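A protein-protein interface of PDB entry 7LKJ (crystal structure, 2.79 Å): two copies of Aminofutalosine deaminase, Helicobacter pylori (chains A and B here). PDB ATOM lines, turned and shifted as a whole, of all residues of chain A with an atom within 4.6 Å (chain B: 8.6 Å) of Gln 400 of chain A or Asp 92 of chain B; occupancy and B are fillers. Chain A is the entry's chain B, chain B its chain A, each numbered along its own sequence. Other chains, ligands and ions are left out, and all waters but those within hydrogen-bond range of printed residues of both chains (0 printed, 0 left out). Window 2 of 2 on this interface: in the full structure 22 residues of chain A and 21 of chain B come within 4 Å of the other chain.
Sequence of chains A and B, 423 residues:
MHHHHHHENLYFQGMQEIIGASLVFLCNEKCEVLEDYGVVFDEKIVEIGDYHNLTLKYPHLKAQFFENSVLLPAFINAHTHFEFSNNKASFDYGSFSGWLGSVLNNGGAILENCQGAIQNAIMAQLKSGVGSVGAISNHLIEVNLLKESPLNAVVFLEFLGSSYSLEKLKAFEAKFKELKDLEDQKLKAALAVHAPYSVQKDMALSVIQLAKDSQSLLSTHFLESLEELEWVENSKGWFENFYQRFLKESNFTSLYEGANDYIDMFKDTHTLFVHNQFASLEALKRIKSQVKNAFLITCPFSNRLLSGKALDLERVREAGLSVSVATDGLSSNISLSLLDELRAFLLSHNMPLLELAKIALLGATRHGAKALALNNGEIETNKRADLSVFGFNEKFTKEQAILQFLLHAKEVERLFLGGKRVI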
ATOM      1  N   LEU A 354     -20.322 -16.561   8.585  1.00  0.00           N
ATOM      2  CA  LEU A 354     -19.694 -16.863   9.866  1.00  0.00           C
ATOM      3  C   LEU A 354     -20.115 -15.882  10.955  1.00  0.00           C
ATOM      4  O   LEU A 354     -20.186 -16.262  12.130  1.00  0.00           O
ATOM      5  CB  LEU A 354     -18.174 -16.880   9.713  1.00  0.00           C
ATOM      6  CG  LEU A 354     -17.620 -18.209   9.193  1.00  0.00           C
ATOM      7  CD1 LEU A 354     -16.236 -18.030   8.587  1.00  0.00           C
ATOM      8  CD2 LEU A 354     -17.598 -19.253  10.300  1.00  0.00           C
ATOM      9  N   PHE A 396     -14.327 -29.923  15.409  1.00  0.00           N
ATOM     10  CA  PHE A 396     -14.369 -28.747  14.554  1.00  0.00           C
ATOM     11  C   PHE A 396     -13.219 -27.834  14.959  1.00  0.00           C
ATOM     12  O   PHE A 396     -12.763 -27.844  16.112  1.00  0.00           O
ATOM     13  CB  PHE A 396     -15.707 -28.006  14.663  1.00  0.00           C
ATOM     14  CG  PHE A 396     -16.902 -28.885  14.569  1.00  0.00           C
ATOM     15  CD1 PHE A 396     -17.007 -29.831  13.557  1.00  0.00           C
ATOM     16  CD2 PHE A 396     -17.908 -28.796  15.506  1.00  0.00           C
ATOM     17  CE1 PHE A 396     -18.113 -30.655  13.485  1.00  0.00           C
ATOM     18  CE2 PHE A 396     -19.008 -29.617  15.439  1.00  0.00           C
ATOM     19  CZ  PHE A 396     -19.109 -30.545  14.429  1.00  0.00           C
ATOM     20  N   THR A 397     -12.716 -27.082  13.989  1.00  0.00           N
ATOM     21  CA  THR A 397     -11.705 -26.086  14.292  1.00  0.00           C
ATOM     22  C   THR A 397     -12.340 -24.931  15.058  1.00  0.00           C
ATOM     23  O   THR A 397     -13.512 -24.603  14.867  1.00  0.00           O
ATOM     24  CB  THR A 397     -11.026 -25.575  13.019  1.00  0.00           C
ATOM     25  OG1 THR A 397     -11.860 -24.599  12.386  1.00  0.00           O
ATOM     26  CG2 THR A 397     -10.768 -26.724  12.045  1.00  0.00           C
ATOM     27  N   LYS A 398     -11.552 -24.325  15.952  1.00  0.00           N
ATOM     28  CA  LYS A 398     -12.073 -23.271  16.820  1.00  0.00           C
ATOM     29  C   LYS A 398     -12.698 -22.121  16.034  1.00  0.00           C
ATOM     30  O   LYS A 398     -13.687 -21.525  16.477  1.00  0.00           O
ATOM     31  CB  LYS A 398     -10.955 -22.748  17.727  1.00  0.00           C
ATOM     32  CG  LYS A 398     -11.178 -21.348  18.295  1.00  0.00           C
ATOM     33  CD  LYS A 398     -10.180 -21.027  19.403  1.00  0.00           C
ATOM     34  CE  LYS A 398      -8.796 -21.579  19.083  1.00  0.00           C
ATOM     35  NZ  LYS A 398      -7.944 -20.588  18.368  1.00  0.00           N
ATOM     36  N   GLU A 399     -12.160 -21.813  14.852  1.00  0.00           N
ATOM     37  CA  GLU A 399     -12.749 -20.759  14.032  1.00  0.00           C
ATOM     38  C   GLU A 399     -14.037 -21.206  13.353  1.00  0.00           C
ATOM     39  O   GLU A 399     -14.853 -20.357  12.971  1.00  0.00           O
ATOM     40  CB  GLU A 399     -11.749 -20.277  12.980  1.00  0.00           C
ATOM     41  CG  GLU A 399     -11.943 -18.830  12.562  1.00  0.00           C
ATOM     42  CD  GLU A 399     -12.749 -18.692  11.284  1.00  0.00           C
ATOM     43  OE1 GLU A 399     -12.630 -19.571  10.405  1.00  0.00           O
ATOM     44  OE2 GLU A 399     -13.505 -17.704  11.159  1.00  0.00           O
ATOM     45  N   GLN A 400     -14.244 -22.513  13.199  1.00  0.00           N
ATOM     46  CA  GLN A 400     -15.415 -23.041  12.515  1.00  0.00           C
ATOM     47  C   GLN A 400     -16.405 -23.727  13.445  1.00  0.00           C
ATOM     48  O   GLN A 400     -17.494 -24.096  12.991  1.00  0.00           O
ATOM     49  CB  GLN A 400     -14.990 -24.032  11.421  1.00  0.00           C
ATOM     50  CG  GLN A 400     -14.277 -23.395  10.242  1.00  0.00           C
ATOM     51  CD  GLN A 400     -15.205 -23.139   9.073  1.00  0.00           C
ATOM     52  OE1 GLN A 400     -16.036 -23.981   8.730  1.00  0.00           O
ATOM     53  NE2 GLN A 400     -15.068 -21.973   8.452  1.00  0.00           N
ATOM     54  N   ALA A 401     -16.060 -23.896  14.725  1.00  0.00           N
ATOM     55  CA  ALA A 401     -16.864 -24.710  15.636  1.00  0.00           C
ATOM     56  C   ALA A 401     -18.323 -24.270  15.656  1.00  0.00           C
ATOM     57  O   ALA A 401     -19.236 -25.099  15.559  1.00  0.00           O
ATOM     58  CB  ALA A 401     -16.268 -24.651  17.043  1.00  0.00           C
ATOM     59  N   ILE A 402     -18.560 -22.964  15.793  1.00  0.00           N
ATOM     60  CA  ILE A 402     -19.926 -22.460  15.933  1.00  0.00           C
ATOM     61  C   ILE A 402     -20.759 -22.797  14.701  1.00  0.00           C
ATOM     62  O   ILE A 402     -21.922 -23.204  14.814  1.00  0.00           O
ATOM     63  CB  ILE A 402     -19.908 -20.946  16.214  1.00  0.00           C
ATOM     64  CG1 ILE A 402     -19.288 -20.671  17.585  1.00  0.00           C
ATOM     65  CG2 ILE A 402     -21.313 -20.368  16.140  1.00  0.00           C
ATOM     66  CD1 ILE A 402     -19.332 -19.217  17.993  1.00  0.00           C
ATOM     67  N   LEU A 403     -20.178 -22.656  13.508  1.00  0.00           N
ATOM     68  CA  LEU A 403     -20.949 -22.896  12.293  1.00  0.00           C
ATOM     69  C   LEU A 403     -21.078 -24.384  11.990  1.00  0.00           C
ATOM     70  O   LEU A 403     -22.143 -24.839  11.556  1.00  0.00           O
ATOM     71  CB  LEU A 403     -20.316 -22.167  11.108  1.00  0.00           C
ATOM     72  CG  LEU A 403     -20.859 -22.548   9.729  1.00  0.00           C
ATOM     73  CD1 LEU A 403     -22.313 -22.114   9.584  1.00  0.00           C
ATOM     74  CD2 LEU A 403     -20.004 -21.951   8.621  1.00  0.00           C
ATOM     75  N   GLN A 404     -20.015 -25.158  12.219  1.00  0.00           N
ATOM     76  CA  GLN A 404     -20.100 -26.597  11.986  1.00  0.00           C
ATOM     77  C   GLN A 404     -21.078 -27.257  12.948  1.00  0.00           C
ATOM     78  O   GLN A 404     -21.662 -28.297  12.622  1.00  0.00           O
ATOM     79  CB  GLN A 404     -18.720 -27.241  12.113  1.00  0.00           C
ATOM     80  CG  GLN A 404     -17.641 -26.619  11.240  1.00  0.00           C
ATOM     81  CD  GLN A 404     -17.748 -27.029   9.786  1.00  0.00           C
ATOM     82  OE1 GLN A 404     -18.473 -27.964   9.442  1.00  0.00           O
ATOM     83  NE2 GLN A 404     -17.019 -26.332   8.922  1.00  0.00           N
ATOM     84  N   ASN B  87     -17.268 -37.033   4.153  1.00  0.00           N
ATOM     85  CA  ASN B  87     -16.891 -35.709   4.643  1.00  0.00           C
ATOM     86  C   ASN B  87     -18.054 -35.097   5.417  1.00  0.00           C
ATOM     87  O   ASN B  87     -18.973 -34.526   4.821  1.00  0.00           O
ATOM     88  CB  ASN B  87     -16.471 -34.812   3.483  1.00  0.00           C
ATOM     89  CG  ASN B  87     -16.075 -33.424   3.934  1.00  0.00           C
ATOM     90  OD1 ASN B  87     -14.931 -33.187   4.315  1.00  0.00           O
ATOM     91  ND2 ASN B  87     -17.021 -32.492   3.888  1.00  0.00           N
ATOM     92  N   LYS B  88     -18.010 -35.208   6.745  1.00  0.00           N
ATOM     93  CA  LYS B  88     -18.988 -34.544   7.601  1.00  0.00           C
ATOM     94  C   LYS B  88     -18.553 -33.115   7.920  1.00  0.00           C
ATOM     95  O   LYS B  88     -19.222 -32.153   7.529  1.00  0.00           O
ATOM     96  CB  LYS B  88     -19.198 -35.350   8.888  1.00  0.00           C
ATOM     97  N   ALA B  89     -17.432 -32.965   8.624  1.00  0.00           N
ATOM     98  CA  ALA B  89     -16.901 -31.643   8.939  1.00  0.00           C
ATOM     99  C   ALA B  89     -15.707 -31.319   8.048  1.00  0.00           C
ATOM    100  O   ALA B  89     -15.880 -30.907   6.895  1.00  0.00           O
ATOM    101  CB  ALA B  89     -16.503 -31.564  10.413  1.00  0.00           C
ATOM    102  N   SER B  90     -14.497 -31.503   8.579  1.00  0.00           N
ATOM    103  CA  SER B  90     -13.253 -31.343   7.832  1.00  0.00           C
ATOM    104  C   SER B  90     -13.114 -29.970   7.177  1.00  0.00           C
ATOM    105  O   SER B  90     -12.306 -29.147   7.619  1.00  0.00           O
ATOM    106  CB  SER B  90     -13.129 -32.437   6.769  1.00  0.00           C
ATOM    107  OG  SER B  90     -12.816 -33.688   7.354  1.00  0.00           O
ATOM    108  N   PHE B  91     -13.891 -29.718   6.126  1.00  0.00           N
ATOM    109  CA  PHE B  91     -13.676 -28.553   5.280  1.00  0.00           C
ATOM    110  C   PHE B  91     -14.216 -27.281   5.929  1.00  0.00           C
ATOM    111  O   PHE B  91     -15.061 -27.314   6.829  1.00  0.00           O
ATOM    112  CB  PHE B  91     -14.326 -28.758   3.911  1.00  0.00           C
ATOM    113  CG  PHE B  91     -13.832 -29.974   3.178  1.00  0.00           C
ATOM    114  CD1 PHE B  91     -12.532 -30.421   3.346  1.00  0.00           C
ATOM    115  CD2 PHE B  91     -14.666 -30.666   2.317  1.00  0.00           C
ATOM    116  CE1 PHE B  91     -12.074 -31.539   2.674  1.00  0.00           C
ATOM    117  CE2 PHE B  91     -14.214 -31.783   1.638  1.00  0.00           C
ATOM    118  CZ  PHE B  91     -12.917 -32.220   1.820  1.00  0.00           C
ATOM    119  N   ASP B  92     -13.710 -26.145   5.449  1.00  0.00           N
ATOM    120  CA  ASP B  92     -14.063 -24.833   5.976  1.00  0.00           C
ATOM    121  C   ASP B  92     -15.198 -24.221   5.164  1.00  0.00           C
ATOM    122  O   ASP B  92     -15.151 -24.213   3.930  1.00  0.00           O
ATOM    123  CB  ASP B  92     -12.851 -23.900   5.950  1.00  0.00           C
ATOM    124  CG  ASP B  92     -11.846 -24.219   7.036  1.00  0.00           C
ATOM    125  OD1 ASP B  92     -11.985 -25.275   7.687  1.00  0.00           O
ATOM    126  OD2 ASP B  92     -10.913 -23.411   7.233  1.00  0.00           O
ATOM    127  N   TYR B  93     -16.213 -23.713   5.856  1.00  0.00           N
ATOM    128  CA  TYR B  93     -17.318 -23.005   5.229  1.00  0.00           C
ATOM    129  C   TYR B  93     -17.318 -21.541   5.651  1.00  0.00           C
ATOM    130  O   TYR B  93     -16.847 -21.188   6.735  1.00  0.00           O
ATOM    131  CB  TYR B  93     -18.657 -23.657   5.579  1.00  0.00           C
ATOM    132  CG  TYR B  93     -18.724 -25.127   5.227  1.00  0.00           C
ATOM    133  CD1 TYR B  93     -18.588 -25.553   3.912  1.00  0.00           C
ATOM    134  CD2 TYR B  93     -18.922 -26.087   6.209  1.00  0.00           C
ATOM    135  CE1 TYR B  93     -18.648 -26.895   3.586  1.00  0.00           C
ATOM    136  CE2 TYR B  93     -18.983 -27.431   5.894  1.00  0.00           C
ATOM    137  CZ  TYR B  93     -18.846 -27.829   4.581  1.00  0.00           C
ATOM    138  OH  TYR B  93     -18.906 -29.167   4.264  1.00  0.00           O
ATOM    139  N   GLY B  94     -17.852 -20.690   4.778  1.00  0.00           N
ATOM    140  CA  GLY B  94     -17.861 -19.251   4.972  1.00  0.00           C
ATOM    141  C   GLY B  94     -17.186 -18.473   3.862  1.00  0.00           C
ATOM    142  O   GLY B  94     -17.391 -17.254   3.754  1.00  0.00           O
ATOM    143  N   SER B  95     -16.377 -19.138   3.043  1.00  0.00           N
ATOM    144  CA  SER B  95     -15.639 -18.514   1.955  1.00  0.00           C
ATOM    145  C   SER B  95     -15.320 -19.598   0.937  1.00  0.00           C
ATOM    146  O   SER B  95     -15.173 -20.770   1.292  1.00  0.00           O
ATOM    147  CB  SER B  95     -14.359 -17.826   2.442  1.00  0.00           C
ATOM    148  OG  SER B  95     -13.637 -18.652   3.337  1.00  0.00           O
ATOM    149  N   PHE B  96     -15.219 -19.202  -0.332  1.00  0.00           N
ATOM    150  CA  PHE B  96     -14.744 -20.148  -1.335  1.00  0.00           C
ATOM    151  C   PHE B  96     -13.239 -20.355  -1.234  1.00  0.00           C
ATOM    152  O   PHE B  96     -12.759 -21.490  -1.342  1.00  0.00           O
ATOM    153  CB  PHE B  96     -15.119 -19.679  -2.739  1.00  0.00           C
ATOM    154  CG  PHE B  96     -14.726 -20.646  -3.820  1.00  0.00           C
ATOM    155  CD1 PHE B  96     -15.459 -21.801  -4.033  1.00  0.00           C
ATOM    156  CD2 PHE B  96     -13.615 -20.408  -4.613  1.00  0.00           C
ATOM    157  CE1 PHE B  96     -15.099 -22.697  -5.023  1.00  0.00           C
ATOM    158  CE2 PHE B  96     -13.249 -21.299  -5.605  1.00  0.00           C
ATOM    159  CZ  PHE B  96     -13.992 -22.446  -5.810  1.00  0.00           C
ATOM    160  N   SER B  97     -12.482 -19.273  -1.036  1.00  0.00           N
ATOM    161  CA  SER B  97     -11.044 -19.402  -0.828  1.00  0.00           C
ATOM    162  C   SER B  97     -10.737 -20.266   0.390  1.00  0.00           C
ATOM    163  O   SER B  97      -9.817 -21.091   0.359  1.00  0.00           O
ATOM    164  CB  SER B  97     -10.414 -18.019  -0.679  1.00  0.00           C
ATOM    165  OG  SER B  97     -11.190 -17.193   0.172  1.00  0.00           O
ATOM    166  N   GLY B  98     -11.496 -20.088   1.472  1.00  0.00           N
ATOM    167  CA  GLY B  98     -11.292 -20.906   2.654  1.00  0.00           C
ATOM    168  C   GLY B  98     -11.662 -22.362   2.454  1.00  0.00           C
ATOM    169  O   GLY B  98     -11.061 -23.248   3.067  1.00  0.00           O
ATOM    170  N   TRP B  99     -12.651 -22.631   1.598  1.00  0.00           N
ATOM    171  CA  TRP B  99     -13.065 -24.008   1.356  1.00  0.00           C
ATOM    172  C   TRP B  99     -12.117 -24.716   0.398  1.00  0.00           C
ATOM    173  O   TRP B  99     -11.760 -25.879   0.620  1.00  0.00           O
ATOM    174  CB  TRP B  99     -14.492 -24.040   0.808  1.00  0.00           C
ATOM    175  CG  TRP B  99     -14.895 -25.375   0.257  1.00  0.00           C
ATOM    176  CD1 TRP B  99     -15.346 -26.451   0.963  1.00  0.00           C
ATOM    177  CD2 TRP B  99     -14.887 -25.772  -1.120  1.00  0.00           C
ATOM    178  NE1 TRP B  99     -15.616 -27.496   0.112  1.00  0.00           N
ATOM    179  CE2 TRP B  99     -15.344 -27.104  -1.172  1.00  0.00           C
ATOM    180  CE3 TRP B  99     -14.537 -25.132  -2.313  1.00  0.00           C
ATOM    181  CZ2 TRP B  99     -15.460 -27.808  -2.370  1.00  0.00           C
ATOM    182  CZ3 TRP B  99     -14.653 -25.832  -3.501  1.00  0.00           C
ATOM    183  CH2 TRP B  99     -15.110 -27.155  -3.520  1.00  0.00           C
ATOM    184  N   LEU B 100     -11.699 -24.034  -0.670  1.00  0.00           N
ATOM    185  CA  LEU B 100     -10.740 -24.630  -1.594  1.00  0.00           C
ATOM    186  C   LEU B 100      -9.384 -24.828  -0.930  1.00  0.00           C
ATOM    187  O   LEU B 100      -8.735 -25.862  -1.128  1.00  0.00           O
ATOM    188  CB  LEU B 100     -10.604 -23.765  -2.846  1.00  0.00           C
ATOM    189  CG  LEU B 100      -9.866 -24.413  -4.018  1.00  0.00           C
ATOM    190  CD1 LEU B 100     -10.397 -25.814  -4.277  1.00  0.00           C
ATOM    191  CD2 LEU B 100      -9.986 -23.553  -5.265  1.00  0.00           C
ATOM    192  N   GLY B 101      -8.938 -23.848  -0.141  1.00  0.00           N
ATOM    193  CA  GLY B 101      -7.696 -24.014   0.597  1.00  0.00           C
ATOM    194  C   GLY B 101      -7.717 -25.216   1.523  1.00  0.00           C
ATOM    195  O   GLY B 101      -6.730 -25.945   1.629  1.00  0.00           O
ATOM    196  N   SER B 102      -8.849 -25.447   2.192  1.00  0.00           N
ATOM    197  CA  SER B 102      -8.972 -26.589   3.090  1.00  0.00           C
ATOM    198  C   SER B 102      -9.157 -27.903   2.343  1.00  0.00           C
ATOM    199  O   SER B 102      -8.872 -28.966   2.906  1.00  0.00           O
ATOM    200  CB  SER B 102     -10.139 -26.377   4.058  1.00  0.00           C
ATOM    201  OG  SER B 102     -11.384 -26.473   3.390  1.00  0.00           O
ATOM    202  N   VAL B 103      -9.626 -27.856   1.096  1.00  0.00           N
ATOM    203  CA  VAL B 103      -9.724 -29.073   0.297  1.00  0.00           C
ATOM    204  C   VAL B 103      -8.360 -29.454  -0.263  1.00  0.00           C
ATOM    205  O   VAL B 103      -8.018 -30.639  -0.350  1.00  0.00           O
ATOM    206  CB  VAL B 103     -10.775 -28.891  -0.815  1.00  0.00           C
ATOM    207  CG1 VAL B 103     -10.591 -29.927  -1.916  1.00  0.00           C
ATOM    208  CG2 VAL B 103     -12.178 -28.975  -0.236  1.00  0.00           C
ATOM    209  N   ASN B 105      -5.416 -28.316   1.128  1.00  0.00           N
ATOM    210  CA  ASN B 105      -4.616 -28.655   2.298  1.00  0.00           C
ATOM    211  C   ASN B 105      -4.893 -30.072   2.779  1.00  0.00           C
ATOM    212  O   ASN B 105      -4.063 -30.649   3.490  1.00  0.00           O
ATOM    213  CB  ASN B 105      -4.878 -27.661   3.431  1.00  0.00           C
ATOM    214  CG  ASN B 105      -3.660 -27.436   4.306  1.00  0.00           C
ATOM    215  OD1 ASN B 105      -2.940 -26.451   4.146  1.00  0.00           O
ATOM    216  ND2 ASN B 105      -3.426 -28.351   5.240  1.00  0.00           N
ATOM    217  N   LEU B 305     -22.812 -22.140   1.917  1.00  0.00           N
ATOM    218  CA  LEU B 305     -21.622 -22.507   2.678  1.00  0.00           C
ATOM    219  C   LEU B 305     -20.361 -21.908   2.065  1.00  0.00           C
ATOM    220  O   LEU B 305     -19.449 -21.494   2.790  1.00  0.00           O
ATOM    221  CB  LEU B 305     -21.509 -24.029   2.762  1.00  0.00           C
ATOM    222  CG  LEU B 305     -22.658 -24.763   3.455  1.00  0.00           C
ATOM    223  CD1 LEU B 305     -22.222 -26.153   3.888  1.00  0.00           C
ATOM    224  CD2 LEU B 305     -23.176 -23.967   4.645  1.00  0.00           C
ATOM    225  N   LEU B 306     -20.287 -21.859   0.736  1.00  0.00           N
ATOM    226  CA  LEU B 306     -19.089 -21.386   0.056  1.00  0.00           C
ATOM    227  C   LEU B 306     -19.143 -19.889  -0.224  1.00  0.00           C
ATOM    228  O   LEU B 306     -18.966 -19.072   0.686  1.00  0.00           O
ATOM    229  CB  LEU B 306     -18.883 -22.153  -1.254  1.00  0.00           C
ATOM    230  CG  LEU B 306     -18.030 -23.423  -1.221  1.00  0.00           C
ATOM    231  CD1 LEU B 306     -18.476 -24.367  -0.115  1.00  0.00           C
ATOM    232  CD2 LEU B 306     -18.067 -24.121  -2.572  1.00  0.00           C
ATOM    233  N   SER B 307     -19.359 -19.535  -1.496  1.00  0.00           N
ATOM    234  CA  SER B 307     -19.420 -18.135  -1.917  1.00  0.00           C
ATOM    235  C   SER B 307     -20.310 -17.291  -1.013  1.00  0.00           C
ATOM    236  O   SER B 307     -19.949 -16.165  -0.652  1.00  0.00           O
ATOM    237  CB  SER B 307     -19.906 -18.051  -3.365  1.00  0.00           C
ATOM    238  OG  SER B 307     -20.131 -19.343  -3.908  1.00  0.00           O
ATOM    239  N   SER B 331     -19.031 -32.590   0.129  1.00  0.00           N
ATOM    240  CA  SER B 331     -17.883 -31.758   0.456  1.00  0.00           C
ATOM    241  C   SER B 331     -18.318 -30.373   0.893  1.00  0.00           C
ATOM    242  O   SER B 331     -17.540 -29.665   1.543  1.00  0.00           O
ATOM    243  CB  SER B 331     -16.946 -31.638  -0.738  1.00  0.00           C
ATOM    244  OG  SER B 331     -16.419 -32.892  -1.118  1.00  0.00           O
ATOM    245  N   SER B 332     -19.547 -29.990   0.549  1.00  0.00           N
ATOM    246  CA  SER B 332     -20.069 -28.653   0.788  1.00  0.00           C
ATOM    247  C   SER B 332     -21.578 -28.728   0.967  1.00  0.00           C
ATOM    248  O   SER B 332     -22.324 -27.871   0.480  1.00  0.00           O
ATOM    249  CB  SER B 332     -19.707 -27.707  -0.358  1.00  0.00           C
ATOM    250  OG  SER B 332     -20.295 -28.139  -1.573  1.00  0.00           O
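The backbone carbonyl oxygen (O) of Phe 91 of chain B lies within hydrogen-bond range of the side-chain amide nitrogen (NE2) of Gln 404 of chain A.
The side-chain amide nitrogen (NE2) of Gln 400 of chain A is in hydrogen-bond range of the backbone carbonyl oxygen (O) of Tyr 93 of chain B, 2.6 Å away.
The side-chain hydroxyl (OG) of Ser 102 of chain B is in hydrogen-bond range of the backbone NH (N) of Asp 92 of chain B.
The backbone carbonyl oxygen (O) of Ser 331 of chain B lies within hydrogen-bond range of the side-chain hydroxyl (OH) of Tyr 93 of chain B (3.1 Å).
The side-chain hydroxyl (OG1) of Thr 397 of chain A sits at hydrogen-bond distance from the backbone NH (N) of Gln 400 of chain A (3.3 Å).
OE1 of Gln 400 of chain A lies within hydrogen-bond range of NE2 of Gln 404 of chain A (2.6 Å).
Among the printed residues, pairs that only touch across the chains: Leu 354 of chain A with Tyr 93 of chain B, Phe 396 of chain A with Ala 89 of chain B, Gln 400 of chain A with Phe 91 of chain B, Gln 400 of chain A with Asp 92 of chain B, Leu 403 of chain A with Tyr 93 of chain B and Gln 404 of chain A with Tyr 93 of chain B.
Of the printed residues of chain B, Gln 400 of chain A touches Phe 91, Asp 92 and Tyr 93.
Asp 92 of chain B touches one residue of chain A.
No residue of chain B comes within 4 Å of Ala 401 of chain A.
Of the printed residues of chain B, Leu 354 of chain A touches Tyr 93.
Printed residues of chain B within 4 Å of Phe 396 of chain A: Ala 89 (3.6 Å).
Of the printed residues of chain A, Phe 91 of chain B touches Gln 400 and Gln 404.
Of the printed residues of chain A, Tyr 93 of chain B touches Leu 354 (3.7 Å), Gln 400 (2.6 Å), Leu 403 (3.7 Å) and Gln 404 (3.3 Å).
The nearest residue of chain B that does not touch Gln 400 of chain A is Gly 94 of chain B (4.8 Å).
The nearest residue of chain A that does not touch Asp 92 of chain B is Gln 404 of chain A (4.4 Å).
The nearest printed residue of chain B that does not touch Gln 404 of chain A is Ala 89 of chain B (4.03 Å).
Of the 10 printed residues of chain A, 5 touch a printed residue of chain B.
Hydrophobic or aromatic side chains of chain B that line the printed part of chain A: Ala 89 and Tyr 93.
Among the printed residues, no Asp or Glu carboxylate lies within 4 Å of a Lys or Arg side-chain nitrogen of the other chain.
No position is printed for both chains.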
